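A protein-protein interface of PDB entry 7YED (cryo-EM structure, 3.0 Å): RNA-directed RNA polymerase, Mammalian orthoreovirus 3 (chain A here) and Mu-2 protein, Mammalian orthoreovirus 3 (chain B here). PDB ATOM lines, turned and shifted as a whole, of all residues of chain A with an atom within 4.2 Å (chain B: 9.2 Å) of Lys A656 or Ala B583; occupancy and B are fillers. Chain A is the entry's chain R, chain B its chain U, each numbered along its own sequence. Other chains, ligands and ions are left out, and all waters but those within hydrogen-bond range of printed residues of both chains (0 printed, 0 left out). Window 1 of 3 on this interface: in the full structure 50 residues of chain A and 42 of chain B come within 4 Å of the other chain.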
ATOM      1  N   GLU A 410      21.491 -21.272   9.402  1.00  0.00           N
ATOM      2  CA  GLU A 410      22.109 -20.293  10.286  1.00  0.00           C
ATOM      3  C   GLU A 410      22.672 -20.920  11.553  1.00  0.00           C
ATOM      4  O   GLU A 410      23.005 -20.192  12.492  1.00  0.00           O
ATOM      5  CB  GLU A 410      21.097 -19.210  10.668  1.00  0.00           C
ATOM      6  CG  GLU A 410      20.614 -18.344   9.521  1.00  0.00           C
ATOM      7  CD  GLU A 410      21.702 -17.458   8.956  1.00  0.00           C
ATOM      8  OE1 GLU A 410      22.598 -17.053   9.726  1.00  0.00           O
ATOM      9  OE2 GLU A 410      21.656 -17.161   7.745  1.00  0.00           O
ATOM     10  N   TRP A 595      25.451 -15.132  22.117  1.00  0.00           N
ATOM     11  CA  TRP A 595      25.481 -16.190  21.118  1.00  0.00           C
ATOM     12  C   TRP A 595      26.671 -17.125  21.266  1.00  0.00           C
ATOM     13  O   TRP A 595      26.588 -18.278  20.834  1.00  0.00           O
ATOM     14  CB  TRP A 595      25.491 -15.588  19.714  1.00  0.00           C
ATOM     15  CG  TRP A 595      25.462 -16.611  18.622  1.00  0.00           C
ATOM     16  CD1 TRP A 595      26.517 -17.044  17.882  1.00  0.00           C
ATOM     17  CD2 TRP A 595      24.320 -17.330  18.148  1.00  0.00           C
ATOM     18  NE1 TRP A 595      26.107 -17.988  16.978  1.00  0.00           N
ATOM     19  CE2 TRP A 595      24.760 -18.181  17.120  1.00  0.00           C
ATOM     20  CE3 TRP A 595      22.967 -17.335  18.492  1.00  0.00           C
ATOM     21  CZ2 TRP A 595      23.900 -19.028  16.434  1.00  0.00           C
ATOM     22  CZ3 TRP A 595      22.114 -18.176  17.809  1.00  0.00           C
ATOM     23  CH2 TRP A 595      22.584 -19.010  16.794  1.00  0.00           C
ATOM     24  N   SER A 652      17.666 -17.173  15.013  1.00  0.00           N
ATOM     25  CA  SER A 652      19.115 -17.245  15.122  1.00  0.00           C
ATOM     26  C   SER A 652      19.776 -16.125  14.337  1.00  0.00           C
ATOM     27  O   SER A 652      20.753 -15.527  14.803  1.00  0.00           O
ATOM     28  CB  SER A 652      19.609 -18.603  14.636  1.00  0.00           C
ATOM     29  OG  SER A 652      19.108 -19.641  15.451  1.00  0.00           O
ATOM     30  N   LEU A 654      18.570 -13.306  13.965  1.00  0.00           N
ATOM     31  CA  LEU A 654      18.416 -12.108  14.790  1.00  0.00           C
ATOM     32  C   LEU A 654      19.398 -12.090  15.958  1.00  0.00           C
ATOM     33  O   LEU A 654      20.037 -11.068  16.220  1.00  0.00           O
ATOM     34  CB  LEU A 654      16.992 -11.987  15.321  1.00  0.00           C
ATOM     35  CG  LEU A 654      16.865 -10.744  16.202  1.00  0.00           C
ATOM     36  CD1 LEU A 654      17.137  -9.493  15.390  1.00  0.00           C
ATOM     37  CD2 LEU A 654      15.507 -10.667  16.865  1.00  0.00           C
ATOM     38  N   TYR A 655      19.515 -13.207  16.683  1.00  0.00           N
ATOM     39  CA  TYR A 655      20.374 -13.240  17.867  1.00  0.00           C
ATOM     40  C   TYR A 655      21.849 -13.100  17.518  1.00  0.00           C
ATOM     41  O   TYR A 655      22.631 -12.631  18.349  1.00  0.00           O
ATOM     42  CB  TYR A 655      20.174 -14.534  18.654  1.00  0.00           C
ATOM     43  CG  TYR A 655      18.861 -14.636  19.384  1.00  0.00           C
ATOM     44  CD1 TYR A 655      18.050 -13.529  19.546  1.00  0.00           C
ATOM     45  CD2 TYR A 655      18.440 -15.839  19.927  1.00  0.00           C
ATOM     46  CE1 TYR A 655      16.849 -13.620  20.215  1.00  0.00           C
ATOM     47  CE2 TYR A 655      17.244 -15.937  20.600  1.00  0.00           C
ATOM     48  CZ  TYR A 655      16.451 -14.826  20.738  1.00  0.00           C
ATOM     49  OH  TYR A 655      15.255 -14.919  21.406  1.00  0.00           O
ATOM     50  N   LYS A 656      22.256 -13.519  16.318  1.00  0.00           N
ATOM     51  CA  LYS A 656      23.674 -13.468  15.980  1.00  0.00           C
ATOM     52  C   LYS A 656      24.184 -12.034  15.918  1.00  0.00           C
ATOM     53  O   LYS A 656      25.278 -11.738  16.411  1.00  0.00           O
ATOM     54  CB  LYS A 656      23.925 -14.178  14.654  1.00  0.00           C
ATOM     55  CG  LYS A 656      23.740 -15.678  14.721  1.00  0.00           C
ATOM     56  CD  LYS A 656      23.833 -16.307  13.349  1.00  0.00           C
ATOM     57  CE  LYS A 656      25.250 -16.284  12.838  1.00  0.00           C
ATOM     58  NZ  LYS A 656      25.358 -16.989  11.539  1.00  0.00           N
ATOM     59  N   ARG A 657      23.410 -11.130  15.323  1.00  0.00           N
ATOM     60  CA  ARG A 657      23.865  -9.757  15.156  1.00  0.00           C
ATOM     61  C   ARG A 657      23.771  -8.939  16.432  1.00  0.00           C
ATOM     62  O   ARG A 657      24.494  -7.950  16.572  1.00  0.00           O
ATOM     63  CB  ARG A 657      23.059  -9.064  14.058  1.00  0.00           C
ATOM     64  CG  ARG A 657      23.458  -7.622  13.831  1.00  0.00           C
ATOM     65  CD  ARG A 657      24.870  -7.543  13.303  1.00  0.00           C
ATOM     66  NE  ARG A 657      25.298  -6.172  13.055  1.00  0.00           N
ATOM     67  CZ  ARG A 657      25.869  -5.394  13.965  1.00  0.00           C
ATOM     68  NH1 ARG A 657      26.084  -5.849  15.187  1.00  0.00           N
ATOM     69  NH2 ARG A 657      26.230  -4.159  13.652  1.00  0.00           N
ATOM     70  N   GLY A 658      22.916  -9.325  17.360  1.00  0.00           N
ATOM     71  CA  GLY A 658      22.632  -8.479  18.492  1.00  0.00           C
ATOM     72  C   GLY A 658      21.443  -7.591  18.211  1.00  0.00           C
ATOM     73  O   GLY A 658      20.782  -7.682  17.173  1.00  0.00           O
ATOM     74  N   VAL B 412      34.759  -8.701   8.819  1.00  0.00           N
ATOM     75  CA  VAL B 412      35.663  -9.460   9.673  1.00  0.00           C
ATOM     76  C   VAL B 412      36.391 -10.490   8.827  1.00  0.00           C
ATOM     77  O   VAL B 412      35.769 -11.221   8.050  1.00  0.00           O
ATOM     78  CB  VAL B 412      34.898 -10.138  10.817  1.00  0.00           C
ATOM     79  CG1 VAL B 412      35.831 -11.026  11.607  1.00  0.00           C
ATOM     80  CG2 VAL B 412      34.266  -9.100  11.714  1.00  0.00           C
ATOM     81  N   ASP B 531      34.708 -11.207  15.078  1.00  0.00           N
ATOM     82  CA  ASP B 531      33.455 -10.493  15.284  1.00  0.00           C
ATOM     83  C   ASP B 531      33.298 -10.000  16.714  1.00  0.00           C
ATOM     84  O   ASP B 531      32.551  -9.046  16.948  1.00  0.00           O
ATOM     85  CB  ASP B 531      32.275 -11.387  14.915  1.00  0.00           C
ATOM     86  CG  ASP B 531      32.217 -12.644  15.750  1.00  0.00           C
ATOM     87  OD1 ASP B 531      33.137 -12.862  16.563  1.00  0.00           O
ATOM     88  OD2 ASP B 531      31.251 -13.418  15.599  1.00  0.00           O
ATOM     89  N   SER B 532      33.962 -10.643  17.675  1.00  0.00           N
ATOM     90  CA  SER B 532      33.864 -10.201  19.060  1.00  0.00           C
ATOM     91  C   SER B 532      34.448  -8.813  19.247  1.00  0.00           C
ATOM     92  O   SER B 532      34.016  -8.079  20.140  1.00  0.00           O
ATOM     93  CB  SER B 532      34.573 -11.189  19.979  1.00  0.00           C
ATOM     94  OG  SER B 532      33.941 -12.449  19.940  1.00  0.00           O
ATOM     95  N   LEU B 534      34.109  -6.328  17.112  1.00  0.00           N
ATOM     96  CA  LEU B 534      33.057  -5.412  16.696  1.00  0.00           C
ATOM     97  C   LEU B 534      31.784  -5.558  17.516  1.00  0.00           C
ATOM     98  O   LEU B 534      30.915  -4.686  17.438  1.00  0.00           O
ATOM     99  CB  LEU B 534      32.738  -5.625  15.217  1.00  0.00           C
ATOM    100  CG  LEU B 534      33.866  -5.326  14.229  1.00  0.00           C
ATOM    101  CD1 LEU B 534      33.452  -5.710  12.823  1.00  0.00           C
ATOM    102  CD2 LEU B 534      34.253  -3.867  14.287  1.00  0.00           C
ATOM    103  N   LEU B 535      31.644  -6.636  18.283  1.00  0.00           N
ATOM    104  CA  LEU B 535      30.462  -6.829  19.110  1.00  0.00           C
ATOM    105  C   LEU B 535      30.649  -6.265  20.513  1.00  0.00           C
ATOM    106  O   LEU B 535      29.765  -5.577  21.029  1.00  0.00           O
ATOM    107  CB  LEU B 535      30.105  -8.316  19.186  1.00  0.00           C
ATOM    108  CG  LEU B 535      29.631  -8.989  17.902  1.00  0.00           C
ATOM    109  CD1 LEU B 535      29.470 -10.476  18.122  1.00  0.00           C
ATOM    110  CD2 LEU B 535      28.329  -8.380  17.437  1.00  0.00           C
ATOM    111  N   LEU B 543      27.541  -5.930   9.893  1.00  0.00           N
ATOM    112  CA  LEU B 543      28.602  -6.816  10.360  1.00  0.00           C
ATOM    113  C   LEU B 543      28.652  -8.014   9.420  1.00  0.00           C
ATOM    114  O   LEU B 543      27.885  -8.967   9.565  1.00  0.00           O
ATOM    115  CB  LEU B 543      28.358  -7.242  11.803  1.00  0.00           C
ATOM    116  CG  LEU B 543      29.484  -7.993  12.504  1.00  0.00           C
ATOM    117  CD1 LEU B 543      29.411  -7.736  13.988  1.00  0.00           C
ATOM    118  CD2 LEU B 543      29.388  -9.475  12.232  1.00  0.00           C
ATOM    119  N   ARG B 545      30.723 -11.062   8.382  1.00  0.00           N
ATOM    120  CA  ARG B 545      31.813 -12.008   8.537  1.00  0.00           C
ATOM    121  C   ARG B 545      32.251 -12.489   7.162  1.00  0.00           C
ATOM    122  O   ARG B 545      31.465 -12.510   6.214  1.00  0.00           O
ATOM    123  CB  ARG B 545      31.380 -13.188   9.400  1.00  0.00           C
ATOM    124  CG  ARG B 545      31.095 -12.820  10.836  1.00  0.00           C
ATOM    125  CD  ARG B 545      30.634 -14.023  11.620  1.00  0.00           C
ATOM    126  NE  ARG B 545      30.362 -13.691  13.012  1.00  0.00           N
ATOM    127  CZ  ARG B 545      29.183 -13.284  13.460  1.00  0.00           C
ATOM    128  NH1 ARG B 545      28.166 -13.152  12.624  1.00  0.00           N
ATOM    129  NH2 ARG B 545      29.021 -13.005  14.743  1.00  0.00           N
ATOM    130  N   LEU B 546      33.518 -12.875   7.048  1.00  0.00           N
ATOM    131  CA  LEU B 546      34.063 -13.239   5.748  1.00  0.00           C
ATOM    132  C   LEU B 546      35.140 -14.298   5.930  1.00  0.00           C
ATOM    133  O   LEU B 546      35.548 -14.614   7.050  1.00  0.00           O
ATOM    134  CB  LEU B 546      34.601 -12.005   5.016  1.00  0.00           C
ATOM    135  CG  LEU B 546      33.537 -10.980   4.613  1.00  0.00           C
ATOM    136  CD1 LEU B 546      34.157  -9.710   4.079  1.00  0.00           C
ATOM    137  CD2 LEU B 546      32.589 -11.572   3.593  1.00  0.00           C
ATOM    138  N   LYS B 547      35.599 -14.847   4.806  1.00  0.00           N
ATOM    139  CA  LYS B 547      36.521 -15.974   4.807  1.00  0.00           C
ATOM    140  C   LYS B 547      37.135 -16.114   3.421  1.00  0.00           C
ATOM    141  O   LYS B 547      36.510 -15.771   2.418  1.00  0.00           O
ATOM    142  CB  LYS B 547      35.802 -17.261   5.214  1.00  0.00           C
ATOM    143  CG  LYS B 547      36.676 -18.486   5.264  1.00  0.00           C
ATOM    144  CD  LYS B 547      35.894 -19.660   5.808  1.00  0.00           C
ATOM    145  CE  LYS B 547      34.857 -20.124   4.808  1.00  0.00           C
ATOM    146  NZ  LYS B 547      34.161 -21.355   5.264  1.00  0.00           N
ATOM    147  N   LYS B 577      41.430 -16.301  16.775  1.00  0.00           N
ATOM    148  CA  LYS B 577      40.521 -17.341  16.307  1.00  0.00           C
ATOM    149  C   LYS B 577      39.809 -18.020  17.466  1.00  0.00           C
ATOM    150  O   LYS B 577      38.685 -18.507  17.306  1.00  0.00           O
ATOM    151  CB  LYS B 577      41.299 -18.358  15.483  1.00  0.00           C
ATOM    152  CG  LYS B 577      40.456 -19.400  14.799  1.00  0.00           C
ATOM    153  CD  LYS B 577      41.344 -20.371  14.053  1.00  0.00           C
ATOM    154  CE  LYS B 577      41.941 -19.714  12.828  1.00  0.00           C
ATOM    155  NZ  LYS B 577      42.722 -20.681  12.018  1.00  0.00           N
ATOM    156  N   ALA B 580      36.435 -15.939  18.939  1.00  0.00           N
ATOM    157  CA  ALA B 580      35.741 -15.716  17.676  1.00  0.00           C
ATOM    158  C   ALA B 580      34.229 -15.915  17.692  1.00  0.00           C
ATOM    159  O   ALA B 580      33.568 -15.423  16.775  1.00  0.00           O
ATOM    160  CB  ALA B 580      36.336 -16.619  16.588  1.00  0.00           C
ATOM    161  N   THR B 581      33.657 -16.617  18.676  1.00  0.00           N
ATOM    162  CA  THR B 581      32.198 -16.752  18.802  1.00  0.00           C
ATOM    163  C   THR B 581      31.587 -17.367  17.541  1.00  0.00           C
ATOM    164  O   THR B 581      30.955 -16.684  16.734  1.00  0.00           O
ATOM    165  CB  THR B 581      31.517 -15.413  19.101  1.00  0.00           C
ATOM    166  OG1 THR B 581      31.631 -14.551  17.965  1.00  0.00           O
ATOM    167  CG2 THR B 581      32.164 -14.752  20.292  1.00  0.00           C
ATOM    168  N   SER B 582      31.837 -18.669  17.387  1.00  0.00           N
ATOM    169  CA  SER B 582      31.620 -19.455  16.174  1.00  0.00           C
ATOM    170  C   SER B 582      30.354 -19.083  15.418  1.00  0.00           C
ATOM    171  O   SER B 582      29.247 -19.156  15.958  1.00  0.00           O
ATOM    172  CB  SER B 582      31.561 -20.932  16.548  1.00  0.00           C
ATOM    173  OG  SER B 582      30.390 -21.193  17.302  1.00  0.00           O
ATOM    174  N   ALA B 583      30.527 -18.705  14.155  1.00  0.00           N
ATOM    175  CA  ALA B 583      29.439 -18.335  13.265  1.00  0.00           C
ATOM    176  C   ALA B 583      29.969 -18.413  11.841  1.00  0.00           C
ATOM    177  O   ALA B 583      31.179 -18.352  11.612  1.00  0.00           O
ATOM    178  CB  ALA B 583      28.896 -16.941  13.585  1.00  0.00           C
ATOM    179  N   GLN B 584      29.064 -18.558  10.891  1.00  0.00           N
ATOM    180  CA  GLN B 584      29.477 -18.844   9.521  1.00  0.00           C
ATOM    181  C   GLN B 584      30.215 -17.672   8.889  1.00  0.00           C
ATOM    182  O   GLN B 584      29.622 -16.604   8.699  1.00  0.00           O
ATOM    183  CB  GLN B 584      28.275 -19.220   8.677  1.00  0.00           C
ATOM    184  CG  GLN B 584      27.735 -20.558   9.059  1.00  0.00           C
ATOM    185  CD  GLN B 584      28.815 -21.605   8.985  1.00  0.00           C
ATOM    186  OE1 GLN B 584      29.238 -22.145  10.004  1.00  0.00           O
ATOM    187  NE2 GLN B 584      29.302 -21.867   7.783  1.00  0.00           N
ATOM    188  N   PRO B 585      31.491 -17.831   8.540  1.00  0.00           N
ATOM    189  CA  PRO B 585      32.220 -16.720   7.910  1.00  0.00           C
ATOM    190  C   PRO B 585      31.683 -16.340   6.540  1.00  0.00           C
ATOM    191  O   PRO B 585      31.674 -15.154   6.199  1.00  0.00           O
ATOM    192  CB  PRO B 585      33.656 -17.252   7.845  1.00  0.00           C
ATOM    193  CG  PRO B 585      33.724 -18.281   8.928  1.00  0.00           C
ATOM    194  CD  PRO B 585      32.384 -18.929   8.931  1.00  0.00           C
ATOM    195  N   LYS B 586      31.250 -17.304   5.733  1.00  0.00           N
ATOM    196  CA  LYS B 586      30.511 -16.992   4.514  1.00  0.00           C
ATOM    197  C   LYS B 586      31.310 -16.231   3.456  1.00  0.00           C
ATOM    198  O   LYS B 586      30.956 -15.102   3.105  1.00  0.00           O
ATOM    199  CB  LYS B 586      29.254 -16.197   4.880  1.00  0.00           C
ATOM    200  CG  LYS B 586      28.281 -15.956   3.739  1.00  0.00           C
ATOM    201  CD  LYS B 586      27.072 -15.177   4.212  1.00  0.00           C
ATOM    202  CE  LYS B 586      26.107 -14.918   3.071  1.00  0.00           C
ATOM    203  NZ  LYS B 586      24.934 -14.126   3.522  1.00  0.00           N
ATOM    204  N   TRP B 587      32.418 -16.811   2.989  1.00  0.00           N
ATOM    205  CA  TRP B 587      32.886 -16.618   1.616  1.00  0.00           C
ATOM    206  C   TRP B 587      33.071 -15.178   1.152  1.00  0.00           C
ATOM    207  O   TRP B 587      32.187 -14.633   0.487  1.00  0.00           O
ATOM    208  CB  TRP B 587      31.974 -17.361   0.647  1.00  0.00           C
ATOM    209  CG  TRP B 587      32.144 -18.805   0.835  1.00  0.00           C
ATOM    210  CD1 TRP B 587      31.227 -19.697   1.303  1.00  0.00           C
ATOM    211  CD2 TRP B 587      33.363 -19.516   0.695  1.00  0.00           C
ATOM    212  NE1 TRP B 587      31.788 -20.949   1.394  1.00  0.00           N
ATOM    213  CE2 TRP B 587      33.109 -20.855   1.031  1.00  0.00           C
ATOM    214  CE3 TRP B 587      34.649 -19.155   0.290  1.00  0.00           C
ATOM    215  CZ2 TRP B 587      34.098 -21.835   0.971  1.00  0.00           C
ATOM    216  CZ3 TRP B 587      35.618 -20.113   0.245  1.00  0.00           C
ATOM    217  CH2 TRP B 587      35.345 -21.444   0.582  1.00  0.00           C
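Hydrophobic or aromatic side chains of chain A that line the printed part of chain B: Trp A595. Printed residues of chain B that touch a printed residue of chain A: Leu B535, Leu B543, Ser B582 and Ala B583. Along chain B the printed residues that touch a printed residue of chain A span positions 535 to 583. Among the printed residues, no Asp or Glu carboxylate lies within 4 Å of a Lys or Arg side-chain nitrogen of the other chain.
Ser B582 touches Trp A595. Lys A656 touches Ala B583 (CE to CB, 3.8 Å). Arg A657 touches Leu B535. CB of Leu B543 touches NE of Arg A657, 3.5 Å away.
Of chain A, only Lys A656 (3.8 Å) comes within 4 Å of Ala B583. Of the printed residues of chain B, Trp A595 touches Ser B582 (3.5 Å). Of the printed residues of chain B, Arg A657 touches Leu B535 and Leu B543. Leu A654 touches none of the printed residues of chain B. The nearest residue of chain B that does not touch Lys A656 is Gln B584 (4.1 Å). The nearest printed residue of chain A that does not touch Ala B583 is Trp A595 (4.5 Å). The nearest printed residue of chain A that does not touch Leu B535 is Lys A656 (4.7 Å).
The side-chain carboxylate of Glu A410 is in salt-bridge range of the side-chain amino group of Lys A656, at 3.3 Å.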
